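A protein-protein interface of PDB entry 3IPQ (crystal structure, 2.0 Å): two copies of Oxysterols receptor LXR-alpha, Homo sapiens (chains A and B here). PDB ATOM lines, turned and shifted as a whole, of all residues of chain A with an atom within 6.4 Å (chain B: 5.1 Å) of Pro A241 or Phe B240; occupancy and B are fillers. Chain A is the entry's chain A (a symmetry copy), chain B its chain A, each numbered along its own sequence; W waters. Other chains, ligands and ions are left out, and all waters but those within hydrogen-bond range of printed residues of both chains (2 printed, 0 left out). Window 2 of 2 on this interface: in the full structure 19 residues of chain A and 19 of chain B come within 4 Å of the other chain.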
ATOM      1  N   HIS A 226      18.334  -4.912  -2.115  1.00  0.00           N
ATOM      2  CA  HIS A 226      16.892  -4.844  -1.929  1.00  0.00           C
ATOM      3  C   HIS A 226      16.525  -4.992  -0.436  1.00  0.00           C
ATOM      4  O   HIS A 226      15.744  -4.213   0.097  1.00  0.00           O
ATOM      5  CB  HIS A 226      16.211  -5.938  -2.757  1.00  0.00           C
ATOM      6  CG  HIS A 226      14.741  -5.741  -2.909  1.00  0.00           C
ATOM      7  ND1 HIS A 226      13.958  -6.569  -3.687  1.00  0.00           N
ATOM      8  CD2 HIS A 226      13.915  -4.791  -2.409  1.00  0.00           C
ATOM      9  CE1 HIS A 226      12.699  -6.162  -3.615  1.00  0.00           C
ATOM     10  NE2 HIS A 226      12.649  -5.085  -2.847  1.00  0.00           N
ATOM     11  N   ASP A 236       9.373   3.531   1.790  1.00  0.00           N
ATOM     12  CA  ASP A 236       9.537   4.017   0.416  1.00  0.00           C
ATOM     13  C   ASP A 236      10.111   2.940  -0.484  1.00  0.00           C
ATOM     14  O   ASP A 236      11.312   2.803  -0.619  1.00  0.00           O
ATOM     15  CB  ASP A 236      10.378   5.293   0.364  1.00  0.00           C
ATOM     16  CG  ASP A 236      10.391   5.913  -1.035  1.00  0.00           C
ATOM     17  OD1 ASP A 236       9.780   5.325  -1.943  1.00  0.00           O
ATOM     18  OD2 ASP A 236      11.013   6.960  -1.234  1.00  0.00           O
ATOM     19  N   ARG A 237       9.209   2.193  -1.102  1.00  0.00           N
ATOM     20  CA  ARG A 237       9.528   1.104  -1.992  1.00  0.00           C
ATOM     21  C   ARG A 237      10.143   1.558  -3.319  1.00  0.00           C
ATOM     22  O   ARG A 237      10.552   0.693  -4.087  1.00  0.00           O
ATOM     23  CB  ARG A 237       8.256   0.323  -2.337  1.00  0.00           C
ATOM     24  CG  ARG A 237       7.738  -0.587  -1.237  1.00  0.00           C
ATOM     25  CD  ARG A 237       6.676  -1.576  -1.793  1.00  0.00           C
ATOM     26  NE  ARG A 237       6.741  -2.898  -1.126  1.00  0.00           N
ATOM     27  CZ  ARG A 237       5.695  -3.568  -0.611  1.00  0.00           C
ATOM     28  NH1 ARG A 237       4.450  -3.070  -0.679  1.00  0.00           N
ATOM     29  NH2 ARG A 237       5.883  -4.768  -0.033  1.00  0.00           N
ATOM     30  N   LEU A 238      10.136   2.862  -3.625  1.00  0.00           N
ATOM     31  CA  LEU A 238      10.791   3.350  -4.826  1.00  0.00           C
ATOM     32  C   LEU A 238      12.291   3.521  -4.672  1.00  0.00           C
ATOM     33  O   LEU A 238      12.979   3.588  -5.663  1.00  0.00           O
ATOM     34  CB  LEU A 238      10.178   4.673  -5.291  1.00  0.00           C
ATOM     35  CG  LEU A 238       8.985   4.459  -6.217  1.00  0.00           C
ATOM     36  CD1 LEU A 238       8.173   5.726  -6.353  1.00  0.00           C
ATOM     37  CD2 LEU A 238       9.494   3.907  -7.588  1.00  0.00           C
ATOM     38  N   MET A 239      12.808   3.594  -3.438  1.00  0.00           N
ATOM     39  CA  MET A 239      14.241   3.830  -3.247  1.00  0.00           C
ATOM     40  C   MET A 239      15.133   2.768  -3.908  1.00  0.00           C
ATOM     41  O   MET A 239      16.105   3.098  -4.545  1.00  0.00           O
ATOM     42  CB  MET A 239      14.572   3.986  -1.750  1.00  0.00           C
ATOM     43  CG  MET A 239      14.049   5.318  -1.220  1.00  0.00           C
ATOM     44  SD  MET A 239      14.704   6.791  -2.035  1.00  0.00           S
ATOM     45  CE  MET A 239      16.482   6.573  -1.897  1.00  0.00           C
ATOM     46  N   PHE A 240      14.783   1.513  -3.766  1.00  0.00           N
ATOM     47  CA  PHE A 240      15.541   0.424  -4.350  1.00  0.00           C
ATOM     48  C   PHE A 240      15.618   0.526  -5.894  1.00  0.00           C
ATOM     49  O   PHE A 240      16.728   0.583  -6.460  1.00  0.00           O
ATOM     50  CB  PHE A 240      14.992  -0.906  -3.876  1.00  0.00           C
ATOM     51  CG  PHE A 240      15.481  -2.106  -4.658  1.00  0.00           C
ATOM     52  CD1 PHE A 240      16.806  -2.423  -4.715  1.00  0.00           C
ATOM     53  CD2 PHE A 240      14.591  -2.891  -5.351  1.00  0.00           C
ATOM     54  CE1 PHE A 240      17.248  -3.504  -5.455  1.00  0.00           C
ATOM     55  CE2 PHE A 240      15.009  -3.989  -6.094  1.00  0.00           C
ATOM     56  CZ  PHE A 240      16.349  -4.305  -6.135  1.00  0.00           C
ATOM     57  N   PRO A 241      14.470   0.525  -6.568  1.00  0.00           N
ATOM     58  CA  PRO A 241      14.595   0.739  -8.019  1.00  0.00           C
ATOM     59  C   PRO A 241      15.245   2.069  -8.460  1.00  0.00           C
ATOM     60  O   PRO A 241      15.896   2.110  -9.509  1.00  0.00           O
ATOM     61  CB  PRO A 241      13.156   0.617  -8.508  1.00  0.00           C
ATOM     62  CG  PRO A 241      12.317   0.844  -7.318  1.00  0.00           C
ATOM     63  CD  PRO A 241      13.060   0.283  -6.179  1.00  0.00           C
ATOM     64  N   ARG A 242      15.071   3.143  -7.696  1.00  0.00           N
ATOM     65  CA  ARG A 242      15.683   4.411  -8.050  1.00  0.00           C
ATOM     66  C   ARG A 242      17.187   4.308  -8.071  1.00  0.00           C
ATOM     67  O   ARG A 242      17.836   4.892  -8.933  1.00  0.00           O
ATOM     68  CB  ARG A 242      15.295   5.526  -7.101  1.00  0.00           C
ATOM     69  CG  ARG A 242      13.917   6.071  -7.298  1.00  0.00           C
ATOM     70  CD  ARG A 242      13.952   7.581  -7.251  1.00  0.00           C
ATOM     71  NE  ARG A 242      13.764   8.052  -5.937  1.00  0.00           N
ATOM     72  CZ  ARG A 242      14.054   9.263  -5.484  1.00  0.00           C
ATOM     73  NH1 ARG A 242      14.625  10.198  -6.219  1.00  0.00           N
ATOM     74  NH2 ARG A 242      13.813   9.500  -4.210  1.00  0.00           N
ATOM     75  N   MET A 243      17.721   3.534  -7.133  1.00  0.00           N
ATOM     76  CA  MET A 243      19.160   3.291  -7.032  1.00  0.00           C
ATOM     77  C   MET A 243      19.637   2.520  -8.199  1.00  0.00           C
ATOM     78  O   MET A 243      20.606   2.920  -8.870  1.00  0.00           O
ATOM     79  CB  MET A 243      19.498   2.500  -5.755  1.00  0.00           C
ATOM     80  CG  MET A 243      19.365   3.344  -4.559  1.00  0.00           C
ATOM     81  SD  MET A 243      19.753   2.409  -3.068  1.00  0.00           S
ATOM     82  CE  MET A 243      18.992   3.505  -1.840  1.00  0.00           C
ATOM     83  N   LEU A 244      18.934   1.426  -8.489  1.00  0.00           N
ATOM     84  CA  LEU A 244      19.256   0.606  -9.669  1.00  0.00           C
ATOM     85  C   LEU A 244      19.225   1.393 -10.960  1.00  0.00           C
ATOM     86  O   LEU A 244      20.077   1.176 -11.828  1.00  0.00           O
ATOM     87  CB  LEU A 244      18.354  -0.635  -9.793  1.00  0.00           C
ATOM     88  CG  LEU A 244      18.501  -1.797  -8.807  1.00  0.00           C
ATOM     89  CD1 LEU A 244      17.529  -2.901  -9.246  1.00  0.00           C
ATOM     90  CD2 LEU A 244      19.941  -2.386  -8.581  1.00  0.00           C
ATOM     91  N   MET A 245      18.280   2.315 -11.086  1.00  0.00           N
ATOM     92  CA  MET A 245      18.119   3.108 -12.307  1.00  0.00           C
ATOM     93  C   MET A 245      19.297   4.076 -12.554  1.00  0.00           C
ATOM     94  O   MET A 245      19.531   4.535 -13.693  1.00  0.00           O
ATOM     95  CB  MET A 245      16.759   3.857 -12.292  1.00  0.00           C
ATOM     96  CG  MET A 245      15.448   2.939 -12.401  1.00  0.00           C
ATOM     97  SD  MET A 245      15.388   2.053 -13.943  1.00  0.00           S
ATOM     98  CE  MET A 245      14.928   3.384 -15.042  1.00  0.00           C
ATOM     99  N   LYS A 246      20.065   4.375 -11.516  1.00  0.00           N
ATOM    100  CA  LYS A 246      21.261   5.200 -11.700  1.00  0.00           C
ATOM    101  C   LYS A 246      22.334   4.492 -12.505  1.00  0.00           C
ATOM    102  O   LYS A 246      23.174   5.149 -13.111  1.00  0.00           O
ATOM    103  CB  LYS A 246      21.814   5.682 -10.343  1.00  0.00           C
ATOM    104  CG  LYS A 246      20.909   6.688  -9.632  1.00  0.00           C
ATOM    105  CD  LYS A 246      20.901   8.048 -10.342  1.00  0.00           C
ATOM    106  CE  LYS A 246      19.825   9.017  -9.796  1.00  0.00           C
ATOM    107  NZ  LYS A 246      18.822   9.337 -10.826  1.00  0.00           N
ATOM    108  N   VAL B 222       7.303   2.269 -12.935  1.00  0.00           N
ATOM    109  CA  VAL B 222       8.137   1.401 -12.099  1.00  0.00           C
ATOM    110  C   VAL B 222       7.309   0.713 -11.009  1.00  0.00           C
ATOM    111  O   VAL B 222       7.440  -0.496 -10.795  1.00  0.00           O
ATOM    112  CB  VAL B 222       9.365   2.174 -11.499  1.00  0.00           C
ATOM    113  CG1 VAL B 222      10.144   1.271 -10.481  1.00  0.00           C
ATOM    114  CG2 VAL B 222      10.310   2.669 -12.640  1.00  0.00           C
ATOM    115  N   LEU B 225       5.015  -1.885 -12.612  1.00  0.00           N
ATOM    116  CA  LEU B 225       5.796  -3.064 -12.949  1.00  0.00           C
ATOM    117  C   LEU B 225       6.129  -3.898 -11.739  1.00  0.00           C
ATOM    118  O   LEU B 225       6.023  -5.106 -11.775  1.00  0.00           O
ATOM    119  CB  LEU B 225       7.081  -2.701 -13.686  1.00  0.00           C
ATOM    120  CG  LEU B 225       7.956  -3.841 -14.227  1.00  0.00           C
ATOM    121  CD1 LEU B 225       7.171  -4.670 -15.271  1.00  0.00           C
ATOM    122  CD2 LEU B 225       9.325  -3.367 -14.812  1.00  0.00           C
ATOM    123  N   HIS B 226       6.510  -3.251 -10.649  1.00  0.00           N
ATOM    124  CA  HIS B 226       6.856  -3.996  -9.448  1.00  0.00           C
ATOM    125  C   HIS B 226       5.649  -4.822  -8.949  1.00  0.00           C
ATOM    126  O   HIS B 226       5.777  -6.004  -8.656  1.00  0.00           O
ATOM    127  CB  HIS B 226       7.329  -3.031  -8.357  1.00  0.00           C
ATOM    128  CG  HIS B 226       8.024  -3.708  -7.225  1.00  0.00           C
ATOM    129  ND1 HIS B 226       8.599  -3.008  -6.183  1.00  0.00           N
ATOM    130  CD2 HIS B 226       8.266  -5.018  -6.985  1.00  0.00           C
ATOM    131  CE1 HIS B 226       9.121  -3.870  -5.323  1.00  0.00           C
ATOM    132  NE2 HIS B 226       8.933  -5.095  -5.789  1.00  0.00           N
ATOM    133  N   VAL B 229       4.662  -7.682 -11.507  1.00  0.00           N
ATOM    134  CA  VAL B 229       5.606  -8.781 -11.517  1.00  0.00           C
ATOM    135  C   VAL B 229       5.454  -9.624 -10.244  1.00  0.00           C
ATOM    136  O   VAL B 229       5.727 -10.785 -10.270  1.00  0.00           O
ATOM    137  CB  VAL B 229       7.061  -8.279 -11.732  1.00  0.00           C
ATOM    138  CG1 VAL B 229       8.105  -9.377 -11.466  1.00  0.00           C
ATOM    139  CG2 VAL B 229       7.213  -7.730 -13.191  1.00  0.00           C
ATOM    140  N   ASP B 236       9.649 -15.292  -7.188  1.00  0.00           N
ATOM    141  CA  ASP B 236      10.962 -14.866  -7.682  1.00  0.00           C
ATOM    142  C   ASP B 236      11.090 -13.354  -7.671  1.00  0.00           C
ATOM    143  O   ASP B 236      10.752 -12.685  -8.628  1.00  0.00           O
ATOM    144  CB  ASP B 236      11.258 -15.440  -9.069  1.00  0.00           C
ATOM    145  CG  ASP B 236      12.698 -15.161  -9.508  1.00  0.00           C
ATOM    146  OD1 ASP B 236      13.425 -14.501  -8.747  1.00  0.00           O
ATOM    147  OD2 ASP B 236      13.095 -15.578 -10.599  1.00  0.00           O
ATOM    148  N   ARG B 237      11.602 -12.849  -6.560  1.00  0.00           N
ATOM    149  CA  ARG B 237      11.801 -11.440  -6.324  1.00  0.00           C
ATOM    150  C   ARG B 237      12.912 -10.827  -7.181  1.00  0.00           C
ATOM    151  O   ARG B 237      13.070  -9.611  -7.131  1.00  0.00           O
ATOM    152  CB  ARG B 237      12.189 -11.205  -4.861  1.00  0.00           C
ATOM    153  CG  ARG B 237      11.049 -11.320  -3.864  1.00  0.00           C
ATOM    154  CD  ARG B 237      11.461 -10.733  -2.484  1.00  0.00           C
ATOM    155  NE  ARG B 237      10.326 -10.072  -1.798  1.00  0.00           N
ATOM    156  CZ  ARG B 237       9.956 -10.278  -0.521  1.00  0.00           C
ATOM    157  NH1 ARG B 237      10.630 -11.129   0.269  1.00  0.00           N
ATOM    158  NH2 ARG B 237       8.906  -9.610  -0.010  1.00  0.00           N
ATOM    159  N   LEU B 238      13.714 -11.639  -7.882  1.00  0.00           N
ATOM    160  CA  LEU B 238      14.719 -11.102  -8.781  1.00  0.00           C
ATOM    161  C   LEU B 238      14.166 -10.687 -10.132  1.00  0.00           C
ATOM    162  O   LEU B 238      14.808  -9.933 -10.823  1.00  0.00           O
ATOM    163  CB  LEU B 238      15.865 -12.096  -8.989  1.00  0.00           C
ATOM    164  CG  LEU B 238      16.954 -11.945  -7.932  1.00  0.00           C
ATOM    165  CD1 LEU B 238      17.862 -13.153  -7.918  1.00  0.00           C
ATOM    166  CD2 LEU B 238      17.721 -10.605  -8.175  1.00  0.00           C
ATOM    167  N   MET B 239      12.979 -11.175 -10.519  1.00  0.00           N
ATOM    168  CA  MET B 239      12.442 -10.856 -11.843  1.00  0.00           C
ATOM    169  C   MET B 239      12.269  -9.351 -12.092  1.00  0.00           C
ATOM    170  O   MET B 239      12.626  -8.859 -13.137  1.00  0.00           O
ATOM    171  CB  MET B 239      11.128 -11.620 -12.097  1.00  0.00           C
ATOM    172  CG  MET B 239      11.403 -13.105 -12.313  1.00  0.00           C
ATOM    173  SD  MET B 239      12.489 -13.503 -13.701  1.00  0.00           S
ATOM    174  CE  MET B 239      11.695 -12.676 -15.084  1.00  0.00           C
ATOM    175  N   PHE B 240      11.744  -8.636 -11.127  1.00  0.00           N
ATOM    176  CA  PHE B 240      11.538  -7.206 -11.242  1.00  0.00           C
ATOM    177  C   PHE B 240      12.865  -6.441 -11.474  1.00  0.00           C
ATOM    178  O   PHE B 240      13.002  -5.726 -12.486  1.00  0.00           O
ATOM    179  CB  PHE B 240      10.765  -6.692 -10.044  1.00  0.00           C
ATOM    180  CG  PHE B 240      10.770  -5.188  -9.886  1.00  0.00           C
ATOM    181  CD1 PHE B 240      10.251  -4.373 -10.849  1.00  0.00           C
ATOM    182  CD2 PHE B 240      11.327  -4.609  -8.770  1.00  0.00           C
ATOM    183  CE1 PHE B 240      10.285  -2.997 -10.710  1.00  0.00           C
ATOM    184  CE2 PHE B 240      11.364  -3.229  -8.604  1.00  0.00           C
ATOM    185  CZ  PHE B 240      10.826  -2.418  -9.578  1.00  0.00           C
ATOM    186  N   PRO B 241      13.815  -6.562 -10.548  1.00  0.00           N
ATOM    187  CA  PRO B 241      15.093  -5.908 -10.873  1.00  0.00           C
ATOM    188  C   PRO B 241      15.804  -6.397 -12.154  1.00  0.00           C
ATOM    189  O   PRO B 241      16.496  -5.607 -12.805  1.00  0.00           O
ATOM    190  CB  PRO B 241      15.932  -6.157  -9.624  1.00  0.00           C
ATOM    191  CG  PRO B 241      15.292  -7.298  -8.944  1.00  0.00           C
ATOM    192  CD  PRO B 241      13.848  -7.170  -9.197  1.00  0.00           C
ATOM    193  N   ARG B 242      15.658  -7.668 -12.514  1.00  0.00           N
ATOM    194  CA  ARG B 242      16.283  -8.172 -13.724  1.00  0.00           C
ATOM    195  C   ARG B 242      15.762  -7.461 -14.947  1.00  0.00           C
ATOM    196  O   ARG B 242      16.522  -7.175 -15.867  1.00  0.00           O
ATOM    197  CB  ARG B 242      16.067  -9.661 -13.909  1.00  0.00           C
ATOM    198  CG  ARG B 242      16.914 -10.533 -13.041  1.00  0.00           C
ATOM    199  CD  ARG B 242      17.489 -11.666 -13.859  1.00  0.00           C
ATOM    200  NE  ARG B 242      16.631 -12.784 -13.850  1.00  0.00           N
ATOM    201  CZ  ARG B 242      16.653 -13.802 -14.698  1.00  0.00           C
ATOM    202  NH1 ARG B 242      17.476 -13.876 -15.726  1.00  0.00           N
ATOM    203  NH2 ARG B 242      15.750 -14.746 -14.525  1.00  0.00           N
ATOM    204  N   MET B 243      14.470  -7.156 -14.926  1.00  0.00           N
ATOM    205  CA  MET B 243      13.809  -6.433 -16.012  1.00  0.00           C
ATOM    206  C   MET B 243      14.323  -5.049 -16.097  1.00  0.00           C
ATOM    207  O   MET B 243      14.738  -4.594 -17.178  1.00  0.00           O
ATOM    208  CB  MET B 243      12.286  -6.373 -15.790  1.00  0.00           C
ATOM    209  CG  MET B 243      11.666  -7.684 -16.032  1.00  0.00           C
ATOM    210  SD  MET B 243       9.885  -7.609 -15.761  1.00  0.00           S
ATOM    211  CE  MET B 243       9.549  -9.383 -15.601  1.00  0.00           C
ATOM    212  N   LEU B 244      14.347  -4.375 -14.948  1.00  0.00           N
ATOM    213  CA  LEU B 244      14.902  -3.013 -14.879  1.00  0.00           C
ATOM    214  C   LEU B 244      16.334  -2.934 -15.359  1.00  0.00           C
ATOM    215  O   LEU B 244      16.699  -1.964 -16.032  1.00  0.00           O
ATOM    216  CB  LEU B 244      14.790  -2.398 -13.472  1.00  0.00           C
ATOM    217  CG  LEU B 244      13.424  -1.990 -12.914  1.00  0.00           C
ATOM    218  CD1 LEU B 244      13.658  -1.341 -11.543  1.00  0.00           C
ATOM    219  CD2 LEU B 244      12.513  -1.074 -13.811  1.00  0.00           C
HETATM  220  O   HOH W   1       8.855  -0.245  -6.218  1.00  0.00           O
HETATM  221  O   HOH W   2      15.048  -8.500  -5.355  1.00  0.00           O
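OD1 of Asp A236 sits at hydrogen-bond distance from N of Leu A238.
Among the printed residues, merely in contact across the chains: Leu A238 with Val B222 (3.97 Å), Phe A240 with Pro B241 (3.97 Å), Pro A241 with Val B222 (3.7 Å), Pro A241 with Phe B240 (3.97 Å), Pro A241 with Leu B244 (3.6 Å) and Leu A244 with Pro B241 (3.6 Å).
Pro A241 touches just these residues of chain B: Val B222 (3.7 Å), Phe B240 (3.97 Å) and Leu B244 (3.6 Å). Of the printed residues of chain B, Leu A244 touches Pro B241 (3.6 Å). Of the printed residues of chain A, Val B222 touches Leu A238 and Pro A241. Phe B240 touches just one residue of chain A: Pro A241. Of the printed residues of chain A, Pro B241 touches Phe A240 (3.97 Å) and Leu A244 (3.6 Å). Of the printed residues of chain A, Leu B244 touches Pro A241 (3.6 Å). The nearest printed residue of chain B that does not touch Pro A241 is His B226 (5.5 Å). The nearest printed residue of chain B that does not touch Leu A244 is Leu B244 (4.8 Å).
Of the 12 printed residues of chain A, 4 touch a printed residue of chain B. Hydrophobic or aromatic side chains of chain A within 4 Å of the printed part of chain B: Leu A238, Phe A240, Pro A241 and Leu A244. Printed residues of chain B that touch a printed residue of chain A: Val B222, Phe B240, Pro B241 and Leu B244. Hydrophobic or aromatic side chains of chain B that line the printed part of chain A: Val B222, Phe B240, Pro B241 and Leu B244. Among the printed residues, no Asp or Glu carboxylate lies within 4 Å of a Lys or Arg side-chain nitrogen of the other chain.
Phe A240 touches Pro B241, and with the chains exchanged Pro A241 touches Phe B240. Pro A241 touches Leu B244, and with the chains exchanged Leu A244 touches Pro B241. Positions printed for both chains: 226, 236, 237, 238, 239, 240, 241, 242, 243 and 244. Of the 6 pairs that touch across the chains among the printed residues, 4 have their exchanged pair printed and touching as well.
Water W1 bridges a ring nitrogen (ND1) of His B226 (2.8 Å) and the backbone carbonyl oxygen of Arg A237 (2.9 Å). Water W2 lies within hydrogen-bond range of a ring nitrogen (ND1) of His A226 and the backbone carbonyl oxygen of Arg B237.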
